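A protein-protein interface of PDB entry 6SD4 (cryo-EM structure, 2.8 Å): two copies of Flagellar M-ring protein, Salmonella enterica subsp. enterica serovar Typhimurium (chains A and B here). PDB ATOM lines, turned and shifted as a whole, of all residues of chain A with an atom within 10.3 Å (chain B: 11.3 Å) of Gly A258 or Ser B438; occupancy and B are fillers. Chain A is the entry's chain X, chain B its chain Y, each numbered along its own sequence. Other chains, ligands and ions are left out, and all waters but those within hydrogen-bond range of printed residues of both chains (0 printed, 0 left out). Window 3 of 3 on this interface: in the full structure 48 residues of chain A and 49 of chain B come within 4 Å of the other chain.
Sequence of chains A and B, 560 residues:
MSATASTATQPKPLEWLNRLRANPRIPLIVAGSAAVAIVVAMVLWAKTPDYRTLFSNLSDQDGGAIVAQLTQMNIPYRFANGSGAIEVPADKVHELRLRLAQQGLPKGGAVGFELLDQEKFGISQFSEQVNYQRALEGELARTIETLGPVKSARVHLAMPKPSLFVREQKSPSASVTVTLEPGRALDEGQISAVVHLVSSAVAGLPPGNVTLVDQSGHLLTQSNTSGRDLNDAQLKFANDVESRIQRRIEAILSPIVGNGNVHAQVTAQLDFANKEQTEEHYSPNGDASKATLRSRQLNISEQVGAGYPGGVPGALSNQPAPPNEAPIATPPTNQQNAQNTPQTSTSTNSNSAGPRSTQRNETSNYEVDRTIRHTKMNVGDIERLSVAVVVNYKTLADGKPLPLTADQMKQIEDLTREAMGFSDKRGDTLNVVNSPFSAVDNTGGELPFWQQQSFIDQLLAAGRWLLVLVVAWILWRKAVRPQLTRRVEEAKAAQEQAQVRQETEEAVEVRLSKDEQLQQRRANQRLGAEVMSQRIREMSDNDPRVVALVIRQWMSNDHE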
ATOM      1  N   ILE A 249      13.047  31.547 -17.144  1.00  0.00           N
ATOM      2  CA  ILE A 249      14.309  30.920 -16.768  1.00  0.00           C
ATOM      3  C   ILE A 249      14.943  30.236 -17.968  1.00  0.00           C
ATOM      4  O   ILE A 249      16.165  30.264 -18.144  1.00  0.00           O
ATOM      5  CB  ILE A 249      14.095  29.935 -15.609  1.00  0.00           C
ATOM      6  CG1 ILE A 249      13.696  30.684 -14.349  1.00  0.00           C
ATOM      7  CG2 ILE A 249      15.347  29.150 -15.351  1.00  0.00           C
ATOM      8  CD1 ILE A 249      13.429  29.798 -13.193  1.00  0.00           C
ATOM      9  N   GLU A 250      14.132  29.604 -18.808  1.00  0.00           N
ATOM     10  CA  GLU A 250      14.675  29.014 -20.018  1.00  0.00           C
ATOM     11  C   GLU A 250      15.111  30.065 -21.022  1.00  0.00           C
ATOM     12  O   GLU A 250      16.112  29.859 -21.711  1.00  0.00           O
ATOM     13  CB  GLU A 250      13.647  28.081 -20.653  1.00  0.00           C
ATOM     14  CG  GLU A 250      13.398  26.812 -19.862  1.00  0.00           C
ATOM     15  CD  GLU A 250      12.030  26.220 -20.131  1.00  0.00           C
ATOM     16  OE1 GLU A 250      11.273  26.811 -20.927  1.00  0.00           O
ATOM     17  OE2 GLU A 250      11.706  25.169 -19.543  1.00  0.00           O
ATOM     18  N   ALA A 251      14.402  31.184 -21.111  1.00  0.00           N
ATOM     19  CA  ALA A 251      14.762  32.241 -22.038  1.00  0.00           C
ATOM     20  C   ALA A 251      16.053  32.949 -21.671  1.00  0.00           C
ATOM     21  O   ALA A 251      16.721  33.481 -22.560  1.00  0.00           O
ATOM     22  CB  ALA A 251      13.636  33.268 -22.134  1.00  0.00           C
ATOM     23  N   ILE A 252      16.429  32.974 -20.396  1.00  0.00           N
ATOM     24  CA  ILE A 252      17.667  33.635 -20.013  1.00  0.00           C
ATOM     25  C   ILE A 252      18.842  32.673 -19.939  1.00  0.00           C
ATOM     26  O   ILE A 252      19.994  33.119 -19.889  1.00  0.00           O
ATOM     27  CB  ILE A 252      17.510  34.375 -18.675  1.00  0.00           C
ATOM     28  CG1 ILE A 252      18.579  35.457 -18.539  1.00  0.00           C
ATOM     29  CG2 ILE A 252      17.617  33.416 -17.524  1.00  0.00           C
ATOM     30  CD1 ILE A 252      18.515  36.491 -19.615  1.00  0.00           C
ATOM     31  N   LEU A 253      18.592  31.369 -19.941  1.00  0.00           N
ATOM     32  CA  LEU A 253      19.678  30.405 -19.949  1.00  0.00           C
ATOM     33  C   LEU A 253      19.899  29.775 -21.312  1.00  0.00           C
ATOM     34  O   LEU A 253      20.982  29.241 -21.558  1.00  0.00           O
ATOM     35  CB  LEU A 253      19.421  29.309 -18.915  1.00  0.00           C
ATOM     36  CG  LEU A 253      19.395  29.777 -17.464  1.00  0.00           C
ATOM     37  CD1 LEU A 253      19.412  28.597 -16.532  1.00  0.00           C
ATOM     38  CD2 LEU A 253      20.570  30.675 -17.188  1.00  0.00           C
ATOM     39  N   SER A 254      18.908  29.832 -22.199  1.00  0.00           N
ATOM     40  CA  SER A 254      19.096  29.304 -23.544  1.00  0.00           C
ATOM     41  C   SER A 254      20.242  29.962 -24.307  1.00  0.00           C
ATOM     42  O   SER A 254      20.954  29.235 -25.020  1.00  0.00           O
ATOM     43  CB  SER A 254      17.788  29.428 -24.336  1.00  0.00           C
ATOM     44  OG  SER A 254      16.713  28.861 -23.620  1.00  0.00           O
ATOM     45  N   PRO A 255      20.463  31.278 -24.243  1.00  0.00           N
ATOM     46  CA  PRO A 255      21.678  31.828 -24.853  1.00  0.00           C
ATOM     47  C   PRO A 255      22.953  31.177 -24.355  1.00  0.00           C
ATOM     48  O   PRO A 255      23.801  30.811 -25.175  1.00  0.00           O
ATOM     49  CB  PRO A 255      21.614  33.306 -24.467  1.00  0.00           C
ATOM     50  CG  PRO A 255      20.177  33.582 -24.402  1.00  0.00           C
ATOM     51  CD  PRO A 255      19.542  32.355 -23.839  1.00  0.00           C
ATOM     52  N   ILE A 256      23.117  31.010 -23.048  1.00  0.00           N
ATOM     53  CA  ILE A 256      24.349  30.436 -22.520  1.00  0.00           C
ATOM     54  C   ILE A 256      24.489  28.978 -22.930  1.00  0.00           C
ATOM     55  O   ILE A 256      25.286  28.633 -23.809  1.00  0.00           O
ATOM     56  CB  ILE A 256      24.405  30.578 -20.992  1.00  0.00           C
ATOM     57  CG1 ILE A 256      24.404  32.044 -20.598  1.00  0.00           C
ATOM     58  CG2 ILE A 256      25.644  29.889 -20.445  1.00  0.00           C
ATOM     59  CD1 ILE A 256      24.621  32.238 -19.141  1.00  0.00           C
ATOM     60  N   VAL A 257      23.716  28.100 -22.295  1.00  0.00           N
ATOM     61  CA  VAL A 257      23.944  26.666 -22.415  1.00  0.00           C
ATOM     62  C   VAL A 257      23.489  26.090 -23.745  1.00  0.00           C
ATOM     63  O   VAL A 257      23.961  25.015 -24.134  1.00  0.00           O
ATOM     64  CB  VAL A 257      23.247  25.915 -21.269  1.00  0.00           C
ATOM     65  CG1 VAL A 257      23.775  26.389 -19.940  1.00  0.00           C
ATOM     66  CG2 VAL A 257      21.755  26.121 -21.346  1.00  0.00           C
ATOM     67  N   GLY A 258      22.594  26.765 -24.454  1.00  0.00           N
ATOM     68  CA  GLY A 258      22.059  26.258 -25.698  1.00  0.00           C
ATOM     69  C   GLY A 258      20.546  26.222 -25.677  1.00  0.00           C
ATOM     70  O   GLY A 258      19.904  26.350 -24.636  1.00  0.00           O
ATOM     71  N   ASN A 259      19.985  26.031 -26.867  1.00  0.00           N
ATOM     72  CA  ASN A 259      18.543  26.156 -27.029  1.00  0.00           C
ATOM     73  C   ASN A 259      17.786  25.128 -26.200  1.00  0.00           C
ATOM     74  O   ASN A 259      16.743  25.451 -25.624  1.00  0.00           O
ATOM     75  CB  ASN A 259      18.167  26.026 -28.502  1.00  0.00           C
ATOM     76  CG  ASN A 259      16.725  26.408 -28.780  1.00  0.00           C
ATOM     77  OD1 ASN A 259      15.964  26.724 -27.868  1.00  0.00           O
ATOM     78  ND2 ASN A 259      16.346  26.386 -30.049  1.00  0.00           N
ATOM     79  N   GLY A 260      18.288  23.902 -26.111  1.00  0.00           N
ATOM     80  CA  GLY A 260      17.560  22.874 -25.396  1.00  0.00           C
ATOM     81  C   GLY A 260      18.382  22.105 -24.388  1.00  0.00           C
ATOM     82  O   GLY A 260      18.102  20.934 -24.127  1.00  0.00           O
ATOM     83  N   ASN A 261      19.396  22.743 -23.813  1.00  0.00           N
ATOM     84  CA  ASN A 261      20.244  22.108 -22.818  1.00  0.00           C
ATOM     85  C   ASN A 261      19.883  22.507 -21.401  1.00  0.00           C
ATOM     86  O   ASN A 261      20.689  22.305 -20.489  1.00  0.00           O
ATOM     87  CB  ASN A 261      21.710  22.436 -23.085  1.00  0.00           C
ATOM     88  CG  ASN A 261      22.144  22.041 -24.466  1.00  0.00           C
ATOM     89  OD1 ASN A 261      21.345  21.558 -25.261  1.00  0.00           O
ATOM     90  ND2 ASN A 261      23.420  22.231 -24.762  1.00  0.00           N
ATOM     91  N   VAL A 262      18.700  23.069 -21.193  1.00  0.00           N
ATOM     92  CA  VAL A 262      18.293  23.526 -19.872  1.00  0.00           C
ATOM     93  C   VAL A 262      16.815  23.230 -19.696  1.00  0.00           C
ATOM     94  O   VAL A 262      16.015  23.415 -20.617  1.00  0.00           O
ATOM     95  CB  VAL A 262      18.607  25.025 -19.674  1.00  0.00           C
ATOM     96  CG1 VAL A 262      17.848  25.873 -20.673  1.00  0.00           C
ATOM     97  CG2 VAL A 262      18.291  25.457 -18.259  1.00  0.00           C
ATOM     98  N   HIS A 263      16.460  22.738 -18.515  1.00  0.00           N
ATOM     99  CA  HIS A 263      15.077  22.483 -18.149  1.00  0.00           C
ATOM    100  C   HIS A 263      14.828  23.035 -16.760  1.00  0.00           C
ATOM    101  O   HIS A 263      15.640  22.842 -15.854  1.00  0.00           O
ATOM    102  CB  HIS A 263      14.750  20.995 -18.177  1.00  0.00           C
ATOM    103  CG  HIS A 263      14.697  20.418 -19.554  1.00  0.00           C
ATOM    104  ND1 HIS A 263      13.548  20.409 -20.311  1.00  0.00           N
ATOM    105  CD2 HIS A 263      15.652  19.831 -20.310  1.00  0.00           C
ATOM    106  CE1 HIS A 263      13.797  19.841 -21.477  1.00  0.00           C
ATOM    107  NE2 HIS A 263      15.067  19.483 -21.501  1.00  0.00           N
ATOM    108  N   VAL A 390      17.904  21.827 -14.391  1.00  0.00           N
ATOM    109  CA  VAL A 390      18.912  20.893 -14.872  1.00  0.00           C
ATOM    110  C   VAL A 390      19.513  21.457 -16.149  1.00  0.00           C
ATOM    111  O   VAL A 390      18.787  21.799 -17.090  1.00  0.00           O
ATOM    112  CB  VAL A 390      18.337  19.484 -15.103  1.00  0.00           C
ATOM    113  CG1 VAL A 390      18.009  18.846 -13.802  1.00  0.00           C
ATOM    114  CG2 VAL A 390      17.097  19.527 -15.960  1.00  0.00           C
ATOM    115  N   VAL A 391      20.835  21.568 -16.176  1.00  0.00           N
ATOM    116  CA  VAL A 391      21.563  22.032 -17.348  1.00  0.00           C
ATOM    117  C   VAL A 391      22.421  20.888 -17.863  1.00  0.00           C
ATOM    118  O   VAL A 391      23.025  20.149 -17.082  1.00  0.00           O
ATOM    119  CB  VAL A 391      22.419  23.278 -17.037  1.00  0.00           C
ATOM    120  CG1 VAL A 391      21.525  24.465 -16.780  1.00  0.00           C
ATOM    121  CG2 VAL A 391      23.294  23.036 -15.833  1.00  0.00           C
ATOM    122  N   ASN A 392      22.458  20.739 -19.182  1.00  0.00           N
ATOM    123  CA  ASN A 392      23.158  19.631 -19.807  1.00  0.00           C
ATOM    124  C   ASN A 392      24.666  19.761 -19.607  1.00  0.00           C
ATOM    125  O   ASN A 392      25.168  20.735 -19.048  1.00  0.00           O
ATOM    126  CB  ASN A 392      22.827  19.580 -21.294  1.00  0.00           C
ATOM    127  CG  ASN A 392      23.042  18.218 -21.890  1.00  0.00           C
ATOM    128  OD1 ASN A 392      23.922  17.477 -21.461  1.00  0.00           O
ATOM    129  ND2 ASN A 392      22.245  17.878 -22.890  1.00  0.00           N
ATOM    130  N   TYR A 393      25.392  18.747 -20.065  1.00  0.00           N
ATOM    131  CA  TYR A 393      26.835  18.868 -20.182  1.00  0.00           C
ATOM    132  C   TYR A 393      27.218  19.502 -21.515  1.00  0.00           C
ATOM    133  O   TYR A 393      26.429  19.565 -22.461  1.00  0.00           O
ATOM    134  CB  TYR A 393      27.518  17.513 -20.037  1.00  0.00           C
ATOM    135  CG  TYR A 393      27.764  17.092 -18.615  1.00  0.00           C
ATOM    136  CD1 TYR A 393      27.543  17.965 -17.568  1.00  0.00           C
ATOM    137  CD2 TYR A 393      28.293  15.848 -18.324  1.00  0.00           C
ATOM    138  CE1 TYR A 393      27.792  17.589 -16.269  1.00  0.00           C
ATOM    139  CE2 TYR A 393      28.547  15.468 -17.031  1.00  0.00           C
ATOM    140  CZ  TYR A 393      28.300  16.343 -16.008  1.00  0.00           C
ATOM    141  OH  TYR A 393      28.556  15.966 -14.714  1.00  0.00           O
ATOM    142  N   LYS A 394      28.458  19.974 -21.582  1.00  0.00           N
ATOM    143  CA  LYS A 394      28.976  20.595 -22.792  1.00  0.00           C
ATOM    144  C   LYS A 394      29.248  19.544 -23.861  1.00  0.00           C
ATOM    145  O   LYS A 394      29.996  18.594 -23.634  1.00  0.00           O
ATOM    146  CB  LYS A 394      30.249  21.387 -22.489  1.00  0.00           C
ATOM    147  CG  LYS A 394      30.695  22.302 -23.617  1.00  0.00           C
ATOM    148  CD  LYS A 394      31.967  23.058 -23.259  1.00  0.00           C
ATOM    149  CE  LYS A 394      33.032  22.896 -24.336  1.00  0.00           C
ATOM    150  NZ  LYS A 394      34.130  23.899 -24.225  1.00  0.00           N
ATOM    151  N   LEU A 404      30.168  21.495 -16.550  1.00  0.00           N
ATOM    152  CA  LEU A 404      30.380  22.930 -16.566  1.00  0.00           C
ATOM    153  C   LEU A 404      31.256  23.331 -15.389  1.00  0.00           C
ATOM    154  O   LEU A 404      31.298  22.655 -14.360  1.00  0.00           O
ATOM    155  CB  LEU A 404      29.043  23.666 -16.512  1.00  0.00           C
ATOM    156  CG  LEU A 404      28.411  24.051 -17.850  1.00  0.00           C
ATOM    157  CD1 LEU A 404      28.329  22.872 -18.793  1.00  0.00           C
ATOM    158  CD2 LEU A 404      27.035  24.637 -17.627  1.00  0.00           C
ATOM    159  N   GLN A 408      31.282  28.795 -13.962  1.00  0.00           N
ATOM    160  CA  GLN A 408      30.245  28.835 -14.984  1.00  0.00           C
ATOM    161  C   GLN A 408      28.907  28.352 -14.442  1.00  0.00           C
ATOM    162  O   GLN A 408      27.863  28.620 -15.045  1.00  0.00           O
ATOM    163  CB  GLN A 408      30.672  27.990 -16.181  1.00  0.00           C
ATOM    164  CG  GLN A 408      29.798  28.127 -17.404  1.00  0.00           C
ATOM    165  CD  GLN A 408      30.380  27.406 -18.601  1.00  0.00           C
ATOM    166  OE1 GLN A 408      31.507  26.913 -18.552  1.00  0.00           O
ATOM    167  NE2 GLN A 408      29.613  27.336 -19.683  1.00  0.00           N
ATOM    168  N   ILE A 412      25.088  30.709 -13.402  1.00  0.00           N
ATOM    169  CA  ILE A 412      23.790  30.198 -13.826  1.00  0.00           C
ATOM    170  C   ILE A 412      22.825  30.193 -12.651  1.00  0.00           C
ATOM    171  O   ILE A 412      21.624  30.430 -12.810  1.00  0.00           O
ATOM    172  CB  ILE A 412      23.945  28.798 -14.443  1.00  0.00           C
ATOM    173  CG1 ILE A 412      24.537  28.906 -15.844  1.00  0.00           C
ATOM    174  CG2 ILE A 412      22.618  28.081 -14.507  1.00  0.00           C
ATOM    175  CD1 ILE A 412      24.522  27.614 -16.600  1.00  0.00           C
ATOM    176  N   PHE A 437      22.158  14.818 -20.347  1.00  0.00           N
ATOM    177  CA  PHE A 437      20.797  14.456 -20.708  1.00  0.00           C
ATOM    178  C   PHE A 437      20.790  13.074 -21.356  1.00  0.00           C
ATOM    179  O   PHE A 437      21.721  12.280 -21.205  1.00  0.00           O
ATOM    180  CB  PHE A 437      20.191  15.516 -21.620  1.00  0.00           C
ATOM    181  CG  PHE A 437      19.814  16.777 -20.910  1.00  0.00           C
ATOM    182  CD1 PHE A 437      20.265  17.032 -19.630  1.00  0.00           C
ATOM    183  CD2 PHE A 437      19.003  17.706 -21.522  1.00  0.00           C
ATOM    184  CE1 PHE A 437      19.919  18.184 -18.986  1.00  0.00           C
ATOM    185  CE2 PHE A 437      18.657  18.855 -20.879  1.00  0.00           C
ATOM    186  CZ  PHE A 437      19.113  19.093 -19.610  1.00  0.00           C
ATOM    187  N   GLY B 260      21.966  41.840 -31.450  1.00  0.00           N
ATOM    188  CA  GLY B 260      21.449  40.658 -30.793  1.00  0.00           C
ATOM    189  C   GLY B 260      22.428  39.971 -29.869  1.00  0.00           C
ATOM    190  O   GLY B 260      22.359  38.755 -29.687  1.00  0.00           O
ATOM    191  N   ASN B 261      23.345  40.731 -29.278  1.00  0.00           N
ATOM    192  CA  ASN B 261      24.326  40.182 -28.357  1.00  0.00           C
ATOM    193  C   ASN B 261      23.963  40.417 -26.905  1.00  0.00           C
ATOM    194  O   ASN B 261      24.827  40.293 -26.033  1.00  0.00           O
ATOM    195  CB  ASN B 261      25.706  40.770 -28.641  1.00  0.00           C
ATOM    196  CG  ASN B 261      26.142  40.549 -30.060  1.00  0.00           C
ATOM    197  OD1 ASN B 261      25.403  39.993 -30.864  1.00  0.00           O
ATOM    198  ND2 ASN B 261      27.356  40.972 -30.377  1.00  0.00           N
ATOM    199  N   VAL B 262      22.712  40.757 -26.621  1.00  0.00           N
ATOM    200  CA  VAL B 262      22.289  41.047 -25.259  1.00  0.00           C
ATOM    201  C   VAL B 262      20.889  40.494 -25.064  1.00  0.00           C
ATOM    202  O   VAL B 262      20.033  40.603 -25.945  1.00  0.00           O
ATOM    203  CB  VAL B 262      22.358  42.560 -24.961  1.00  0.00           C
ATOM    204  CG1 VAL B 262      21.427  43.334 -25.871  1.00  0.00           C
ATOM    205  CG2 VAL B 262      22.031  42.834 -23.509  1.00  0.00           C
ATOM    206  N   HIS B 263      20.669  39.870 -23.912  1.00  0.00           N
ATOM    207  CA  HIS B 263      19.365  39.361 -23.526  1.00  0.00           C
ATOM    208  C   HIS B 263      19.084  39.767 -22.093  1.00  0.00           C
ATOM    209  O   HIS B 263      19.953  39.653 -21.228  1.00  0.00           O
ATOM    210  CB  HIS B 263      19.289  37.843 -23.655  1.00  0.00           C
ATOM    211  CG  HIS B 263      19.276  37.360 -25.067  1.00  0.00           C
ATOM    212  ND1 HIS B 263      18.115  37.210 -25.791  1.00  0.00           N
ATOM    213  CD2 HIS B 263      20.284  36.997 -25.893  1.00  0.00           C
ATOM    214  CE1 HIS B 263      18.408  36.773 -27.001  1.00  0.00           C
ATOM    215  NE2 HIS B 263      19.718  36.636 -27.089  1.00  0.00           N
ATOM    216  N   VAL B 390      22.412  38.938 -19.910  1.00  0.00           N
ATOM    217  CA  VAL B 390      23.541  38.222 -20.487  1.00  0.00           C
ATOM    218  C   VAL B 390      23.987  38.965 -21.736  1.00  0.00           C
ATOM    219  O   VAL B 390      23.176  39.243 -22.627  1.00  0.00           O
ATOM    220  CB  VAL B 390      23.200  36.755 -20.805  1.00  0.00           C
ATOM    221  CG1 VAL B 390      23.036  35.984 -19.546  1.00  0.00           C
ATOM    222  CG2 VAL B 390      21.936  36.647 -21.619  1.00  0.00           C
ATOM    223  N   VAL B 391      25.270  39.300 -21.793  1.00  0.00           N
ATOM    224  CA  VAL B 391      25.863  39.958 -22.948  1.00  0.00           C
ATOM    225  C   VAL B 391      26.876  39.013 -23.572  1.00  0.00           C
ATOM    226  O   VAL B 391      27.628  38.336 -22.864  1.00  0.00           O
ATOM    227  CB  VAL B 391      26.510  41.306 -22.571  1.00  0.00           C
ATOM    228  CG1 VAL B 391      25.442  42.306 -22.201  1.00  0.00           C
ATOM    229  CG2 VAL B 391      27.462  41.135 -21.414  1.00  0.00           C
ATOM    230  N   ASN B 392      26.885  38.963 -24.898  1.00  0.00           N
ATOM    231  CA  ASN B 392      27.733  38.034 -25.623  1.00  0.00           C
ATOM    232  C   ASN B 392      29.205  38.403 -25.458  1.00  0.00           C
ATOM    233  O   ASN B 392      29.561  39.409 -24.843  1.00  0.00           O
ATOM    234  CB  ASN B 392      27.353  38.028 -27.100  1.00  0.00           C
ATOM    235  CG  ASN B 392      27.769  36.767 -27.800  1.00  0.00           C
ATOM    236  OD1 ASN B 392      28.776  36.157 -27.452  1.00  0.00           O
ATOM    237  ND2 ASN B 392      26.999  36.366 -28.799  1.00  0.00           N
ATOM    238  N   TYR B 393      30.071  37.560 -26.009  1.00  0.00           N
ATOM    239  CA  TYR B 393      31.467  37.930 -26.159  1.00  0.00           C
ATOM    240  C   TYR B 393      31.685  38.709 -27.452  1.00  0.00           C
ATOM    241  O   TYR B 393      30.859  38.702 -28.367  1.00  0.00           O
ATOM    242  CB  TYR B 393      32.371  36.703 -26.135  1.00  0.00           C
ATOM    243  CG  TYR B 393      32.742  36.234 -24.755  1.00  0.00           C
ATOM    244  CD1 TYR B 393      32.422  36.984 -23.641  1.00  0.00           C
ATOM    245  CD2 TYR B 393      33.482  35.081 -24.573  1.00  0.00           C
ATOM    246  CE1 TYR B 393      32.783  36.569 -22.380  1.00  0.00           C
ATOM    247  CE2 TYR B 393      33.848  34.662 -23.320  1.00  0.00           C
ATOM    248  CZ  TYR B 393      33.501  35.412 -22.226  1.00  0.00           C
ATOM    249  OH  TYR B 393      33.869  34.996 -20.972  1.00  0.00           O
ATOM    250  N   ASN B 434      28.724  37.926 -18.435  1.00  0.00           N
ATOM    251  CA  ASN B 434      29.311  37.944 -19.763  1.00  0.00           C
ATOM    252  C   ASN B 434      29.735  36.530 -20.131  1.00  0.00           C
ATOM    253  O   ASN B 434      30.595  35.946 -19.466  1.00  0.00           O
ATOM    254  CB  ASN B 434      30.503  38.896 -19.801  1.00  0.00           C
ATOM    255  CG  ASN B 434      30.931  39.227 -21.198  1.00  0.00           C
ATOM    256  OD1 ASN B 434      30.136  39.192 -22.133  1.00  0.00           O
ATOM    257  ND2 ASN B 434      32.199  39.548 -21.355  1.00  0.00           N
ATOM    258  N   SER B 435      29.132  35.979 -21.183  1.00  0.00           N
ATOM    259  CA  SER B 435      29.431  34.618 -21.564  1.00  0.00           C
ATOM    260  C   SER B 435      29.029  34.376 -23.009  1.00  0.00           C
ATOM    261  O   SER B 435      28.010  34.917 -23.459  1.00  0.00           O
ATOM    262  CB  SER B 435      28.717  33.620 -20.652  1.00  0.00           C
ATOM    263  OG  SER B 435      27.328  33.883 -20.616  1.00  0.00           O
ATOM    264  N   PRO B 436      29.784  33.568 -23.747  1.00  0.00           N
ATOM    265  CA  PRO B 436      29.531  33.433 -25.185  1.00  0.00           C
ATOM    266  C   PRO B 436      28.234  32.699 -25.471  1.00  0.00           C
ATOM    267  O   PRO B 436      27.887  31.723 -24.804  1.00  0.00           O
ATOM    268  CB  PRO B 436      30.740  32.637 -25.681  1.00  0.00           C
ATOM    269  CG  PRO B 436      31.182  31.872 -24.495  1.00  0.00           C
ATOM    270  CD  PRO B 436      30.898  32.721 -23.299  1.00  0.00           C
ATOM    271  N   PHE B 437      27.526  33.169 -26.488  1.00  0.00           N
ATOM    272  CA  PHE B 437      26.231  32.607 -26.835  1.00  0.00           C
ATOM    273  C   PHE B 437      26.428  31.293 -27.583  1.00  0.00           C
ATOM    274  O   PHE B 437      27.483  30.658 -27.518  1.00  0.00           O
ATOM    275  CB  PHE B 437      25.421  33.609 -27.647  1.00  0.00           C
ATOM    276  CG  PHE B 437      24.868  34.737 -26.836  1.00  0.00           C
ATOM    277  CD1 PHE B 437      25.323  34.978 -25.554  1.00  0.00           C
ATOM    278  CD2 PHE B 437      23.890  35.555 -27.354  1.00  0.00           C
ATOM    279  CE1 PHE B 437      24.816  36.007 -24.817  1.00  0.00           C
ATOM    280  CE2 PHE B 437      23.384  36.584 -26.620  1.00  0.00           C
ATOM    281  CZ  PHE B 437      23.845  36.808 -25.348  1.00  0.00           C
ATOM    282  N   SER B 438      25.399  30.867 -28.303  1.00  0.00           N
ATOM    283  CA  SER B 438      25.454  29.626 -29.054  1.00  0.00           C
ATOM    284  C   SER B 438      25.103  29.876 -30.514  1.00  0.00           C
ATOM    285  O   SER B 438      23.994  30.302 -30.829  1.00  0.00           O
ATOM    286  CB  SER B 438      24.508  28.593 -28.443  1.00  0.00           C
ATOM    287  OG  SER B 438      24.940  28.222 -27.146  1.00  0.00           O
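Of chain B, only Ser B438 comes within 4 Å of Gly A258. Of the printed residues of chain A, Ser B438 touches Pro A255, Ile A256 and Gly A258. Pro A255 touches just these residues of chain B: His B263 (3.7 Å), Phe B437 (3.4 Å) and Ser B438 (3.4 Å). No residue of chain B comes within 4 Å of Val A257. No residue of chain B comes within 4 Å of Asn A259. No residue of chain B comes within 4 Å of Gly A260. No residue of chain B comes within 4 Å of Asn A261. No residue of chain B comes within 4 Å of Val A262. Of the printed residues of chain A, Val B390 touches Ile A252 (3.97 Å). Of the printed residues of chain A, Phe B437 touches Pro A255 (3.4 Å). Printed residues of chain B within 4 Å of Ile A256: Ser B435 and Ser B438. The nearest printed residue of chain A that does not touch Ser B435 is Pro A255 (6.1 Å).
The backbone carbonyl oxygen (O) of Pro A255 is in hydrogen-bond range of the side-chain hydroxyl (OG) of Ser B438, at 3.4 Å. The backbone carbonyl oxygen (O) of Ile A256 is in hydrogen-bond range of the side-chain hydroxyl (OG) of Ser B438 (3.4 Å).
Printed residues of chain A that touch a printed residue of chain B: Ile A252, Pro A255, Ile A256 and Gly A258. Hydrophobic or aromatic side chains of chain A that line the printed part of chain B: Ile A252, Pro A255 and Ile A256. Of the 13 printed residues of chain B, 5 touch a printed residue of chain A. Printed residues of chain B that touch a printed residue of chain A: His B263, Val B390, Ser B435, Phe B437 and Ser B438. Hydrophobic or aromatic side chains of chain B within 4 Å of the printed part of chain A: His B263 and Val B390. Among the printed residues, no Asp or Glu carboxylate lies within 4 Å of a Lys or Arg side-chain nitrogen of the other chain.
Among the printed residues, pairs that only touch across the chains: Ile A252 with His B263 (3.8 Å), Ile A252 with Val B390 (3.97 Å), Pro A255 with His B263 (3.7 Å), Pro A255 with Phe B437 (3.4 Å), Ile A256 with Ser B435 (3.5 Å) and Gly A258 with Ser B438 (3.8 Å).
The backbone NH (N) of Val B390 is in hydrogen-bond range of the backbone carbonyl oxygen (O) of His B263 (2.9 Å). O of Val B391 sits at hydrogen-bond distance from N of Ser B435 (3.3 Å). The side-chain amide oxygen (OD1) of Asn B392 sits at hydrogen-bond distance from the backbone NH (N) of Phe B437 (3.4 Å).
9 positions are printed for both chains.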
